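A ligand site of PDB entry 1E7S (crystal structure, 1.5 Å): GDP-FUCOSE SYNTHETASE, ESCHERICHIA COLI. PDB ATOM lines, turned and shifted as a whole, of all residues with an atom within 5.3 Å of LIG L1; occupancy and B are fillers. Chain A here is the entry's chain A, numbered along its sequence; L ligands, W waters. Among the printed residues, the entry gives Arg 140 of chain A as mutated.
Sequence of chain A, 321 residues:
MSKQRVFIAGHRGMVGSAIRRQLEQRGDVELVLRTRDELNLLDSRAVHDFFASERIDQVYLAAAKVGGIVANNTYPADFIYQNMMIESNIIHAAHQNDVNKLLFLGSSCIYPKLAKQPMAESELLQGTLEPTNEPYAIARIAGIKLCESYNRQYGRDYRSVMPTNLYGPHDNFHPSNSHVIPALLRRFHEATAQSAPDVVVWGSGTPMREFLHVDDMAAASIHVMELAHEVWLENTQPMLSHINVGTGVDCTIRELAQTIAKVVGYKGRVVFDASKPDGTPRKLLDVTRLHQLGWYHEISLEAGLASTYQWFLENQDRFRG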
ATOM      1  N   GLY A  10      21.003   4.729  15.750  1.00  0.00           N
ATOM      2  CA  GLY A  10      20.633   3.389  16.198  1.00  0.00           C
ATOM      3  C   GLY A  10      19.145   3.231  16.457  1.00  0.00           C
ATOM      4  O   GLY A  10      18.774   2.476  17.330  1.00  0.00           O
ATOM      5  N   HIS A  11      18.314   3.931  15.717  1.00  0.00           N
ATOM      6  CA  HIS A  11      16.880   3.988  16.003  1.00  0.00           C
ATOM      7  C   HIS A  11      16.113   2.690  15.879  1.00  0.00           C
ATOM      8  O   HIS A  11      14.983   2.605  16.391  1.00  0.00           O
ATOM      9  CB  HIS A  11      16.159   5.114  15.224  1.00  0.00           C
ATOM     10  CG  HIS A  11      15.959   4.735  13.783  1.00  0.00           C
ATOM     11  ND1 HIS A  11      17.015   4.823  12.876  1.00  0.00           N
ATOM     12  CD2 HIS A  11      14.867   4.319  13.102  1.00  0.00           C
ATOM     13  CE1 HIS A  11      16.565   4.410  11.678  1.00  0.00           C
ATOM     14  NE2 HIS A  11      15.264   4.159  11.793  1.00  0.00           N
ATOM     15  N   ARG A  12      16.672   1.669  15.200  1.00  0.00           N
ATOM     16  CA  ARG A  12      15.983   0.388  15.104  1.00  0.00           C
ATOM     17  C   ARG A  12      16.405  -0.571  16.212  1.00  0.00           C
ATOM     18  O   ARG A  12      15.929  -1.691  16.291  1.00  0.00           O
ATOM     19  CB  ARG A  12      16.256  -0.272  13.745  1.00  0.00           C
ATOM     20  CG  ARG A  12      15.670   0.495  12.563  1.00  0.00           C
ATOM     21  CD  ARG A  12      15.536  -0.313  11.300  1.00  0.00           C
ATOM     22  NE  ARG A  12      14.597   0.340  10.372  1.00  0.00           N
ATOM     23  CZ  ARG A  12      14.547  -0.070   9.096  1.00  0.00           C
ATOM     24  NH1 ARG A  12      15.395  -1.018   8.707  1.00  0.00           N
ATOM     25  NH2 ARG A  12      13.716   0.490   8.238  1.00  0.00           N
ATOM     26  N   GLY A  13      17.339  -0.132  17.049  1.00  0.00           N
ATOM     27  CA  GLY A  13      17.814  -0.998  18.134  1.00  0.00           C
ATOM     28  C   GLY A  13      16.779  -1.086  19.266  1.00  0.00           C
ATOM     29  O   GLY A  13      15.776  -0.360  19.284  1.00  0.00           O
ATOM     30  N   MET A  14      17.060  -1.927  20.252  1.00  0.00           N
ATOM     31  CA  MET A  14      16.150  -2.109  21.370  1.00  0.00           C
ATOM     32  C   MET A  14      15.962  -0.807  22.125  1.00  0.00           C
ATOM     33  O   MET A  14      14.832  -0.328  22.311  1.00  0.00           O
ATOM     34  CB  MET A  14      16.631  -3.221  22.352  1.00  0.00           C
ATOM     35  CG  MET A  14      15.434  -3.679  23.254  1.00  0.00           C
ATOM     36  SD  MET A  14      16.138  -4.939  24.333  1.00  0.00           S
ATOM     37  CE  MET A  14      14.779  -4.933  25.458  1.00  0.00           C
ATOM     38  N   VAL A  15      17.056  -0.137  22.486  1.00  0.00           N
ATOM     39  CA  VAL A  15      16.935   1.154  23.211  1.00  0.00           C
ATOM     40  C   VAL A  15      16.519   2.256  22.252  1.00  0.00           C
ATOM     41  O   VAL A  15      15.662   3.084  22.601  1.00  0.00           O
ATOM     42  CB  VAL A  15      18.305   1.442  23.896  1.00  0.00           C
ATOM     43  CG1 VAL A  15      18.363   2.839  24.443  1.00  0.00           C
ATOM     44  CG2 VAL A  15      18.561   0.475  25.060  1.00  0.00           C
ATOM     45  N   GLY A  16      17.191   2.367  21.107  1.00  0.00           N
ATOM     46  CA  GLY A  16      16.860   3.469  20.191  1.00  0.00           C
ATOM     47  C   GLY A  16      15.411   3.503  19.759  1.00  0.00           C
ATOM     48  O   GLY A  16      14.777   4.573  19.661  1.00  0.00           O
ATOM     49  N   THR A  35      18.768   4.493   8.642  1.00  0.00           N
ATOM     50  CA  THR A  35      19.078   3.097   8.887  1.00  0.00           C
ATOM     51  C   THR A  35      20.585   2.869   8.644  1.00  0.00           C
ATOM     52  O   THR A  35      21.295   3.740   8.120  1.00  0.00           O
ATOM     53  CB  THR A  35      18.265   2.215   7.918  1.00  0.00           C
ATOM     54  OG1 THR A  35      18.792   2.453   6.613  1.00  0.00           O
ATOM     55  CG2 THR A  35      16.769   2.438   8.004  1.00  0.00           C
ATOM     56  N   ARG A  36      21.104   1.719   9.096  1.00  0.00           N
ATOM     57  CA  ARG A  36      22.506   1.396   8.829  1.00  0.00           C
ATOM     58  C   ARG A  36      22.784   1.482   7.323  1.00  0.00           C
ATOM     59  O   ARG A  36      23.910   1.789   6.919  1.00  0.00           O
ATOM     60  CB  ARG A  36      22.854   0.013   9.364  1.00  0.00           C
ATOM     61  CG  ARG A  36      24.294  -0.403   9.257  1.00  0.00           C
ATOM     62  CD  ARG A  36      24.708  -1.572  10.169  1.00  0.00           C
ATOM     63  NE  ARG A  36      26.149  -1.791  10.017  1.00  0.00           N
ATOM     64  CZ  ARG A  36      26.874  -2.428  10.928  1.00  0.00           C
ATOM     65  NH1 ARG A  36      26.189  -2.865  11.972  1.00  0.00           N
ATOM     66  NH2 ARG A  36      28.182  -2.622  10.765  1.00  0.00           N
ATOM     67  N   LEU A  39      23.254   5.025   6.429  1.00  0.00           N
ATOM     68  CA  LEU A  39      24.372   5.704   7.069  1.00  0.00           C
ATOM     69  C   LEU A  39      25.124   4.718   7.963  1.00  0.00           C
ATOM     70  O   LEU A  39      24.674   4.288   9.028  1.00  0.00           O
ATOM     71  CB  LEU A  39      23.876   6.899   7.899  1.00  0.00           C
ATOM     72  CG  LEU A  39      24.964   7.626   8.741  1.00  0.00           C
ATOM     73  CD1 LEU A  39      26.077   8.190   7.873  1.00  0.00           C
ATOM     74  CD2 LEU A  39      24.325   8.741   9.555  1.00  0.00           C
ATOM     75  N   ASN A  40      26.341   4.382   7.494  1.00  0.00           N
ATOM     76  CA  ASN A  40      27.237   3.510   8.237  1.00  0.00           C
ATOM     77  C   ASN A  40      28.014   4.368   9.234  1.00  0.00           C
ATOM     78  O   ASN A  40      28.882   5.170   8.884  1.00  0.00           O
ATOM     79  CB  ASN A  40      28.171   2.751   7.348  1.00  0.00           C
ATOM     80  CG  ASN A  40      29.162   1.821   8.016  1.00  0.00           C
ATOM     81  OD1 ASN A  40      29.962   1.154   7.329  1.00  0.00           O
ATOM     82  ND2 ASN A  40      29.116   1.718   9.299  1.00  0.00           N
ATOM     83  N   LEU A  41      27.694   4.205  10.507  1.00  0.00           N
ATOM     84  CA  LEU A  41      28.239   5.028  11.559  1.00  0.00           C
ATOM     85  C   LEU A  41      29.726   4.837  11.814  1.00  0.00           C
ATOM     86  O   LEU A  41      30.323   5.617  12.540  1.00  0.00           O
ATOM     87  CB  LEU A  41      27.425   5.014  12.844  1.00  0.00           C
ATOM     88  CG  LEU A  41      25.956   5.429  12.695  1.00  0.00           C
ATOM     89  CD1 LEU A  41      25.161   4.958  13.907  1.00  0.00           C
ATOM     90  CD2 LEU A  41      25.823   6.931  12.480  1.00  0.00           C
ATOM     91  N   LEU A  42      30.276   3.762  11.257  1.00  0.00           N
ATOM     92  CA  LEU A  42      31.709   3.538  11.301  1.00  0.00           C
ATOM     93  C   LEU A  42      32.461   4.395  10.283  1.00  0.00           C
ATOM     94  O   LEU A  42      33.678   4.528  10.478  1.00  0.00           O
ATOM     95  CB  LEU A  42      32.015   2.076  10.972  1.00  0.00           C
ATOM     96  CG  LEU A  42      31.439   1.062  11.966  1.00  0.00           C
ATOM     97  CD1 LEU A  42      31.430  -0.341  11.350  1.00  0.00           C
ATOM     98  CD2 LEU A  42      32.209   1.084  13.284  1.00  0.00           C
ATOM     99  N   ALA A  62      22.379   6.019  20.583  1.00  0.00           N
ATOM    100  CA  ALA A  62      21.941   4.698  20.919  1.00  0.00           C
ATOM    101  C   ALA A  62      22.435   3.621  19.952  1.00  0.00           C
ATOM    102  O   ALA A  62      22.021   2.446  20.011  1.00  0.00           O
ATOM    103  CB  ALA A  62      20.391   4.690  20.952  1.00  0.00           C
ATOM    104  N   ALA A  63      23.306   3.961  19.001  1.00  0.00           N
ATOM    105  CA  ALA A  63      23.918   2.984  18.110  1.00  0.00           C
ATOM    106  C   ALA A  63      25.160   2.347  18.775  1.00  0.00           C
ATOM    107  O   ALA A  63      25.962   3.047  19.368  1.00  0.00           O
ATOM    108  CB  ALA A  63      24.381   3.621  16.817  1.00  0.00           C
ATOM    109  N   ALA A  64      25.255   1.031  18.646  1.00  0.00           N
ATOM    110  CA  ALA A  64      26.352   0.286  19.277  1.00  0.00           C
ATOM    111  C   ALA A  64      26.385  -1.126  18.727  1.00  0.00           C
ATOM    112  O   ALA A  64      25.385  -1.636  18.200  1.00  0.00           O
ATOM    113  CB  ALA A  64      26.160   0.252  20.788  1.00  0.00           C
ATOM    114  N   LYS A  65      27.531  -1.759  18.874  1.00  0.00           N
ATOM    115  CA  LYS A  65      27.698  -3.203  18.635  1.00  0.00           C
ATOM    116  C   LYS A  65      27.582  -3.901  19.994  1.00  0.00           C
ATOM    117  O   LYS A  65      28.410  -3.645  20.868  1.00  0.00           O
ATOM    118  CB  LYS A  65      29.073  -3.400  17.978  1.00  0.00           C
ATOM    119  CG  LYS A  65      29.520  -4.820  17.852  1.00  0.00           C
ATOM    120  CD  LYS A  65      28.505  -5.685  17.156  1.00  0.00           C
ATOM    121  CE  LYS A  65      29.222  -7.031  16.815  1.00  0.00           C
ATOM    122  NZ  LYS A  65      28.320  -7.980  16.139  1.00  0.00           N
ATOM    123  N   VAL A  66      26.484  -4.626  20.178  1.00  0.00           N
ATOM    124  CA  VAL A  66      26.113  -5.194  21.480  1.00  0.00           C
ATOM    125  C   VAL A  66      25.789  -6.660  21.272  1.00  0.00           C
ATOM    126  O   VAL A  66      25.297  -7.086  20.221  1.00  0.00           O
ATOM    127  CB  VAL A  66      24.860  -4.488  22.045  1.00  0.00           C
ATOM    128  CG1 VAL A  66      24.478  -4.958  23.434  1.00  0.00           C
ATOM    129  CG2 VAL A  66      25.155  -2.986  22.140  1.00  0.00           C
ATOM    130  N   GLY A  67      26.198  -7.459  22.277  1.00  0.00           N
ATOM    131  CA  GLY A  67      25.974  -8.893  22.191  1.00  0.00           C
ATOM    132  C   GLY A  67      26.054  -9.526  23.589  1.00  0.00           C
ATOM    133  O   GLY A  67      26.260  -8.827  24.591  1.00  0.00           O
ATOM    134  N   GLY A  68      25.925 -10.845  23.605  1.00  0.00           N
ATOM    135  CA  GLY A  68      25.973 -11.596  24.842  1.00  0.00           C
ATOM    136  C   GLY A  68      27.333 -12.177  25.158  1.00  0.00           C
ATOM    137  O   GLY A  68      28.371 -11.715  24.666  1.00  0.00           O
ATOM    138  N   GLN A  82      34.433  -1.324  16.933  1.00  0.00           N
ATOM    139  CA  GLN A  82      33.227  -0.686  16.348  1.00  0.00           C
ATOM    140  C   GLN A  82      32.643   0.352  17.261  1.00  0.00           C
ATOM    141  O   GLN A  82      32.200   1.417  16.802  1.00  0.00           O
ATOM    142  CB  GLN A  82      32.188  -1.754  15.986  1.00  0.00           C
ATOM    143  CG  GLN A  82      32.652  -2.651  14.850  1.00  0.00           C
ATOM    144  CD  GLN A  82      31.703  -3.749  14.452  1.00  0.00           C
ATOM    145  OE1 GLN A  82      30.476  -3.562  14.595  1.00  0.00           O
ATOM    146  NE2 GLN A  82      32.191  -4.897  13.996  1.00  0.00           N
ATOM    147  N   ILE A  86      32.182   4.275  16.312  1.00  0.00           N
ATOM    148  CA  ILE A  86      30.839   4.899  16.234  1.00  0.00           C
ATOM    149  C   ILE A  86      30.774   6.126  17.155  1.00  0.00           C
ATOM    150  O   ILE A  86      30.361   7.226  16.784  1.00  0.00           O
ATOM    151  CB  ILE A  86      29.775   3.870  16.691  1.00  0.00           C
ATOM    152  CG1 ILE A  86      29.670   2.757  15.618  1.00  0.00           C
ATOM    153  CG2 ILE A  86      28.451   4.549  16.945  1.00  0.00           C
ATOM    154  CD1 ILE A  86      28.822   1.564  16.056  1.00  0.00           C
ATOM    155  N   ARG A 140      32.976   1.546  25.938  1.00  0.00           N
ATOM    156  CA  ARG A 140      31.905   2.327  26.576  1.00  0.00           C
ATOM    157  C   ARG A 140      32.455   3.449  27.453  1.00  0.00           C
ATOM    158  O   ARG A 140      31.968   4.605  27.497  1.00  0.00           O
ATOM    159  CB  ARG A 140      30.904   1.449  27.292  1.00  0.00           C
ATOM    160  CG  ARG A 140      30.068   0.530  26.389  1.00  0.00           C
ATOM    161  CD  ARG A 140      29.275   1.347  25.385  1.00  0.00           C
ATOM    162  NE  ARG A 140      27.988   0.732  25.046  1.00  0.00           N
ATOM    163  CZ  ARG A 140      27.053   1.300  24.304  1.00  0.00           C
ATOM    164  NH1 ARG A 140      27.288   2.436  23.673  1.00  0.00           N
ATOM    165  NH2 ARG A 140      25.833   0.702  24.169  1.00  0.00           N
ATOM    166  N   LEU A 166      18.445  -4.642  30.901  1.00  0.00           N
ATOM    167  CA  LEU A 166      17.193  -4.234  30.242  1.00  0.00           C
ATOM    168  C   LEU A 166      16.426  -5.412  29.703  1.00  0.00           C
ATOM    169  O   LEU A 166      16.965  -6.468  29.390  1.00  0.00           O
ATOM    170  CB  LEU A 166      17.520  -3.316  29.042  1.00  0.00           C
ATOM    171  CG  LEU A 166      18.245  -2.018  29.408  1.00  0.00           C
ATOM    172  CD1 LEU A 166      18.594  -1.238  28.140  1.00  0.00           C
ATOM    173  CD2 LEU A 166      17.366  -1.172  30.353  1.00  0.00           C
ATOM    174  N   ASP A 171      13.609  -7.242  21.977  1.00  0.00           N
ATOM    175  CA  ASP A 171      14.745  -8.020  22.472  1.00  0.00           C
ATOM    176  C   ASP A 171      14.898  -9.257  21.581  1.00  0.00           C
ATOM    177  O   ASP A 171      14.100  -9.545  20.697  1.00  0.00           O
ATOM    178  CB  ASP A 171      14.486  -8.402  23.933  1.00  0.00           C
ATOM    179  CG  ASP A 171      15.742  -8.534  24.742  1.00  0.00           C
ATOM    180  OD1 ASP A 171      16.858  -8.685  24.173  1.00  0.00           O
ATOM    181  OD2 ASP A 171      15.642  -8.562  25.987  1.00  0.00           O
ATOM    182  N   ASN A 172      15.955 -10.025  21.817  1.00  0.00           N
ATOM    183  CA  ASN A 172      16.200 -11.300  21.136  1.00  0.00           C
ATOM    184  C   ASN A 172      15.651 -12.464  21.945  1.00  0.00           C
ATOM    185  O   ASN A 172      16.305 -12.918  22.919  1.00  0.00           O
ATOM    186  CB  ASN A 172      17.715 -11.439  20.925  1.00  0.00           C
ATOM    187  CG  ASN A 172      18.154 -12.718  20.245  1.00  0.00           C
ATOM    188  OD1 ASN A 172      19.346 -13.059  20.222  1.00  0.00           O
ATOM    189  ND2 ASN A 172      17.212 -13.432  19.631  1.00  0.00           N
ATOM    190  N   ASN A 177      19.923 -17.020  24.255  1.00  0.00           N
ATOM    191  CA  ASN A 177      20.362 -15.663  24.653  1.00  0.00           C
ATOM    192  C   ASN A 177      20.984 -15.801  26.028  1.00  0.00           C
ATOM    193  O   ASN A 177      20.410 -16.405  26.958  1.00  0.00           O
ATOM    194  CB  ASN A 177      19.128 -14.737  24.597  1.00  0.00           C
ATOM    195  CG  ASN A 177      19.486 -13.259  24.732  1.00  0.00           C
ATOM    196  OD1 ASN A 177      20.431 -12.858  25.414  1.00  0.00           O
ATOM    197  ND2 ASN A 177      18.687 -12.366  24.172  1.00  0.00           N
ATOM    198  N   SER A 178      22.134 -15.151  26.265  1.00  0.00           N
ATOM    199  CA  SER A 178      22.733 -15.128  27.600  1.00  0.00           C
ATOM    200  C   SER A 178      22.054 -14.173  28.574  1.00  0.00           C
ATOM    201  O   SER A 178      22.338 -14.217  29.757  1.00  0.00           O
ATOM    202  CB  SER A 178      24.232 -14.890  27.577  1.00  0.00           C
ATOM    203  OG  SER A 178      24.524 -13.653  26.986  1.00  0.00           O
ATOM    204  N   HIS A 179      21.183 -13.296  28.130  1.00  0.00           N
ATOM    205  CA  HIS A 179      20.393 -12.422  28.971  1.00  0.00           C
ATOM    206  C   HIS A 179      19.185 -13.205  29.493  1.00  0.00           C
ATOM    207  O   HIS A 179      18.401 -13.764  28.716  1.00  0.00           O
ATOM    208  CB  HIS A 179      19.921 -11.159  28.253  1.00  0.00           C
ATOM    209  CG  HIS A 179      20.980 -10.277  27.718  1.00  0.00           C
ATOM    210  ND1 HIS A 179      21.551 -10.469  26.478  1.00  0.00           N
ATOM    211  CD2 HIS A 179      21.693  -9.296  28.307  1.00  0.00           C
ATOM    212  CE1 HIS A 179      22.514  -9.587  26.294  1.00  0.00           C
ATOM    213  NE2 HIS A 179      22.650  -8.888  27.385  1.00  0.00           N
HETATM  214  P1  LIG L   1      20.903  -3.023  19.684  1.00  0.00           P
HETATM  215  O1  LIG L   1      21.795  -3.977  19.020  1.00  0.00           O
HETATM  216  O2  LIG L   1      19.479  -3.510  19.907  1.00  0.00           O
HETATM  217  O3  LIG L   1      20.846  -1.667  18.959  1.00  0.00           O
HETATM  218  C1  LIG L   1      22.068  -1.112  18.390  1.00  0.00           C
HETATM  219  C2  LIG L   1      21.589  -0.395  17.072  1.00  0.00           C
HETATM  220  O4  LIG L   1      22.821   0.209  16.514  1.00  0.00           O
HETATM  221  C3  LIG L   1      21.143  -1.429  15.989  1.00  0.00           C
HETATM  222  O5  LIG L   1      19.999  -0.932  15.322  1.00  0.00           O
HETATM  223  C4  LIG L   1      22.356  -1.510  15.046  1.00  0.00           C
HETATM  224  O6  LIG L   1      22.018  -1.767  13.669  1.00  0.00           O
HETATM  225  C5  LIG L   1      22.847  -0.089  15.133  1.00  0.00           C
HETATM  226  N1  LIG L   1      24.216   0.049  14.684  1.00  0.00           N
HETATM  227  C6  LIG L   1      25.288  -0.689  15.113  1.00  0.00           C
HETATM  228  N2  LIG L   1      26.348  -0.417  14.375  1.00  0.00           N
HETATM  229  C7  LIG L   1      25.941   0.487  13.396  1.00  0.00           C
HETATM  230  C8  LIG L   1      26.619   1.103  12.304  1.00  0.00           C
HETATM  231  N3  LIG L   1      27.899   0.780  11.967  1.00  0.00           N
HETATM  232  N4  LIG L   1      25.923   1.991  11.556  1.00  0.00           N
HETATM  233  C9  LIG L   1      24.624   2.252  11.860  1.00  0.00           C
HETATM  234  N5  LIG L   1      23.886   1.635  12.812  1.00  0.00           N
HETATM  235  C10 LIG L   1      24.637   0.850  13.642  1.00  0.00           C
HETATM  236  O7  LIG L   1      21.532  -2.654  20.998  1.00  0.00           O
HETATM  237  P2  LIG L   1      20.977  -1.873  22.342  1.00  0.00           P
HETATM  238  O8  LIG L   1      19.725  -1.149  21.969  1.00  0.00           O
HETATM  239  O9  LIG L   1      22.097  -1.056  23.006  1.00  0.00           O
HETATM  240  O10 LIG L   1      20.561  -3.078  23.190  1.00  0.00           O
HETATM  241  C11 LIG L   1      19.979  -2.882  24.484  1.00  0.00           C
HETATM  242  C12 LIG L   1      19.815  -4.238  25.126  1.00  0.00           C
HETATM  243  O11 LIG L   1      19.193  -5.063  24.133  1.00  0.00           O
HETATM  244  C13 LIG L   1      21.140  -5.022  25.322  1.00  0.00           C
HETATM  245  O12 LIG L   1      21.583  -4.558  26.605  1.00  0.00           O
HETATM  246  C14 LIG L   1      20.460  -6.405  25.593  1.00  0.00           C
HETATM  247  O13 LIG L   1      19.619  -6.265  26.774  1.00  0.00           O
HETATM  248  C15 LIG L   1      19.572  -6.404  24.406  1.00  0.00           C
HETATM  249  N6  LIG L   1      20.440  -6.827  23.359  1.00  0.00           N
HETATM  250  C16 LIG L   1      20.975  -8.115  23.433  1.00  0.00           C
HETATM  251  C17 LIG L   1      21.774  -8.646  22.407  1.00  0.00           C
HETATM  252  C18 LIG L   1      22.405 -10.050  22.474  1.00  0.00           C
HETATM  253  O14 LIG L   1      22.331 -10.658  23.583  1.00  0.00           O
HETATM  254  N7  LIG L   1      22.842 -10.577  21.257  1.00  0.00           N
HETATM  255  C19 LIG L   1      21.951  -7.883  21.245  1.00  0.00           C
HETATM  256  C20 LIG L   1      21.368  -6.572  21.160  1.00  0.00           C
HETATM  257  C21 LIG L   1      20.553  -6.113  22.242  1.00  0.00           C
HETATM  258  P3  LIG L   1      22.256  -3.171  13.040  1.00  0.00           P
HETATM  259  O15 LIG L   1      21.825  -2.993  11.615  1.00  0.00           O
HETATM  260  O16 LIG L   1      23.695  -3.610  13.310  1.00  0.00           O
HETATM  261  O17 LIG L   1      21.518  -4.144  13.842  1.00  0.00           O
HETATM  262  C1  LG2 L   2      25.694 -14.856  23.771  1.00  0.00           C
HETATM  263  O1  LG2 L   2      26.318 -15.596  24.532  1.00  0.00           O
HETATM  264  C2  LG2 L   2      24.445 -14.633  23.729  1.00  0.00           C
HETATM  265  O2  LG2 L   2      26.548 -13.777  22.964  1.00  0.00           O
HETATM  266  P1  LG2 L   2      25.634 -13.628  21.805  1.00  0.00           P
HETATM  267  O3  LG2 L   2      25.498 -12.275  21.357  1.00  0.00           O
HETATM  268  O4  LG2 L   2      26.353 -14.294  20.743  1.00  0.00           O
HETATM  269  O5  LG2 L   2      24.268 -14.427  21.873  1.00  0.00           O
HETATM  270  O   HOH W   1      23.637  -1.073  25.192  1.00  0.00           O
HETATM  271  O   HOH W   2      18.990  -3.150  14.217  1.00  0.00           O
HETATM  272  O   HOH W   3      19.473   0.990  20.257  1.00  0.00           O
HETATM  273  O   HOH W   4      19.223   1.220  13.861  1.00  0.00           O
HETATM  274  O   HOH W   5      24.414  -4.286  18.040  1.00  0.00           O
HETATM  275  O   HOH W   6      23.221   1.355  22.843  1.00  0.00           O
HETATM  276  O   HOH W   7      22.652   4.767  10.748  1.00  0.00           O
HETATM  277  O   HOH W   8      25.411  -4.180  15.301  1.00  0.00           O
HETATM  278  O   HOH W   9      22.513  -9.931  18.065  1.00  0.00           O
HETATM  279  O   HOH W  10      21.804  -5.302  16.290  1.00  0.00           O
HETATM  280  O   HOH W  11      18.299  -5.254  18.615  1.00  0.00           O
HETATM  281  O   HOH W  12      19.042  -9.707  24.900  1.00  0.00           O
HETATM  282  O   HOH W  13      21.310   2.639  12.915  1.00  0.00           O
HETATM  283  O   HOH W  14      20.744  -5.483  29.302  1.00  0.00           O
HETATM  284  O   HOH W  15      17.812  -8.369  27.533  1.00  0.00           O
HETATM  285  O   HOH W  16      28.987  -1.355  13.671  1.00  0.00           O
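An oxygen (O3) of LG2 L2 is in hydrogen-bond range of a nitrogen (N7) of LIG L1.
Merely in contact with LIG L1: Gly 10 (3.9 Å), Arg 12 (3.7 Å), Leu 39 (3.5 Å), Leu 42 (3.6 Å), Ala 62 (3.9 Å), Ala 63 (3.4 Å), Val 66 (3.6 Å), Gly 67 (3.7 Å), Gly 68 (3.6 Å), Ile 86 (3.6 Å), Leu 166 (3.7 Å) and Asp 171 (3.6 Å). Hydrophobic or aromatic side chains that line LIG L1: Met 14, Val 15, Leu 41, Leu 42, Ala 63, Val 66, Ile 86 and His 179. The nearest printed residue that does not touch LIG L1 is Arg 140 (4.3 Å).
Water W1 lies within hydrogen-bond range of O9 of LIG L1 (2.7 Å) and NH2 of Arg 140 (3.0 Å). Water W4 lies within hydrogen-bond range of O5 of LIG L1 (2.7 Å), N of Arg 12 (2.9 Å) and N of His 11 (3.4 Å). Water W3 lies within hydrogen-bond range of O8 of LIG L1 (2.8 Å), N of Gly 16 (2.8 Å), O of Ala 62 (2.9 Å), O of Gly 10 (3.4 Å) and N of Val 15 (3.5 Å). Water W5 lies within hydrogen-bond range of O1 of LIG L1, O of Ala 64 and N of Val 66. Water W14 bridges O13 of LIG L1 (2.9 Å) and N of Leu 166 (2.9 Å). Water W15 lies within hydrogen-bond range of the side-chain carboxylate (OD2) of Asp 171 (2.7 Å), the backbone carbonyl oxygen (O) of Leu 166 (2.8 Å) and an oxygen (O13) of LIG L1 (2.9 Å).
The backbone NH of Leu 41 sits at hydrogen-bond distance from a nitrogen (N4) of LIG L1 (3.0 Å). The side-chain amide oxygen (OD1) of Asn 177 sits close to an oxygen (O14) of LIG L1, at 3.4 Å. An oxygen (O14) of LIG L1 sits close to a ring nitrogen (ND1) of His 179 (3.0 Å). The backbone NH (N) of Gly 13 lies within hydrogen-bond range of an oxygen (O5) of LIG L1 (3.3 Å). The backbone NH (N) of Met 14 is in hydrogen-bond range of an oxygen (O2) of LIG L1 (2.9 Å). NH1 of Arg 36 lies within salt-bridge range of O16 of LIG L1. The backbone NH of Gly 68 sits at hydrogen-bond distance from an oxygen (O3) of LG2 L2 (2.7 Å). The backbone NH of Ala 64 sits at hydrogen-bond distance from an oxygen (O4) of LIG L1 (3.3 Å). A nitrogen (N3) of LIG L1 sits close to the side-chain amide nitrogen of Asn 40 (3.1 Å). The backbone NH of Val 15 is in hydrogen-bond range of an oxygen (O8) of LIG L1 (2.9 Å).
A ring nitrogen (ND1) of His 179 lies within hydrogen-bond range of the side-chain amide oxygen (OD1) of Asn 177. The side-chain amide nitrogen (ND2) of Asn 177 sits at hydrogen-bond distance from the backbone carbonyl oxygen (O) of Asn 172 (2.7 Å). The backbone NH (N) of Leu 42 lies close to the side-chain amide nitrogen (ND2) of Asn 40, at 3.1 Å.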
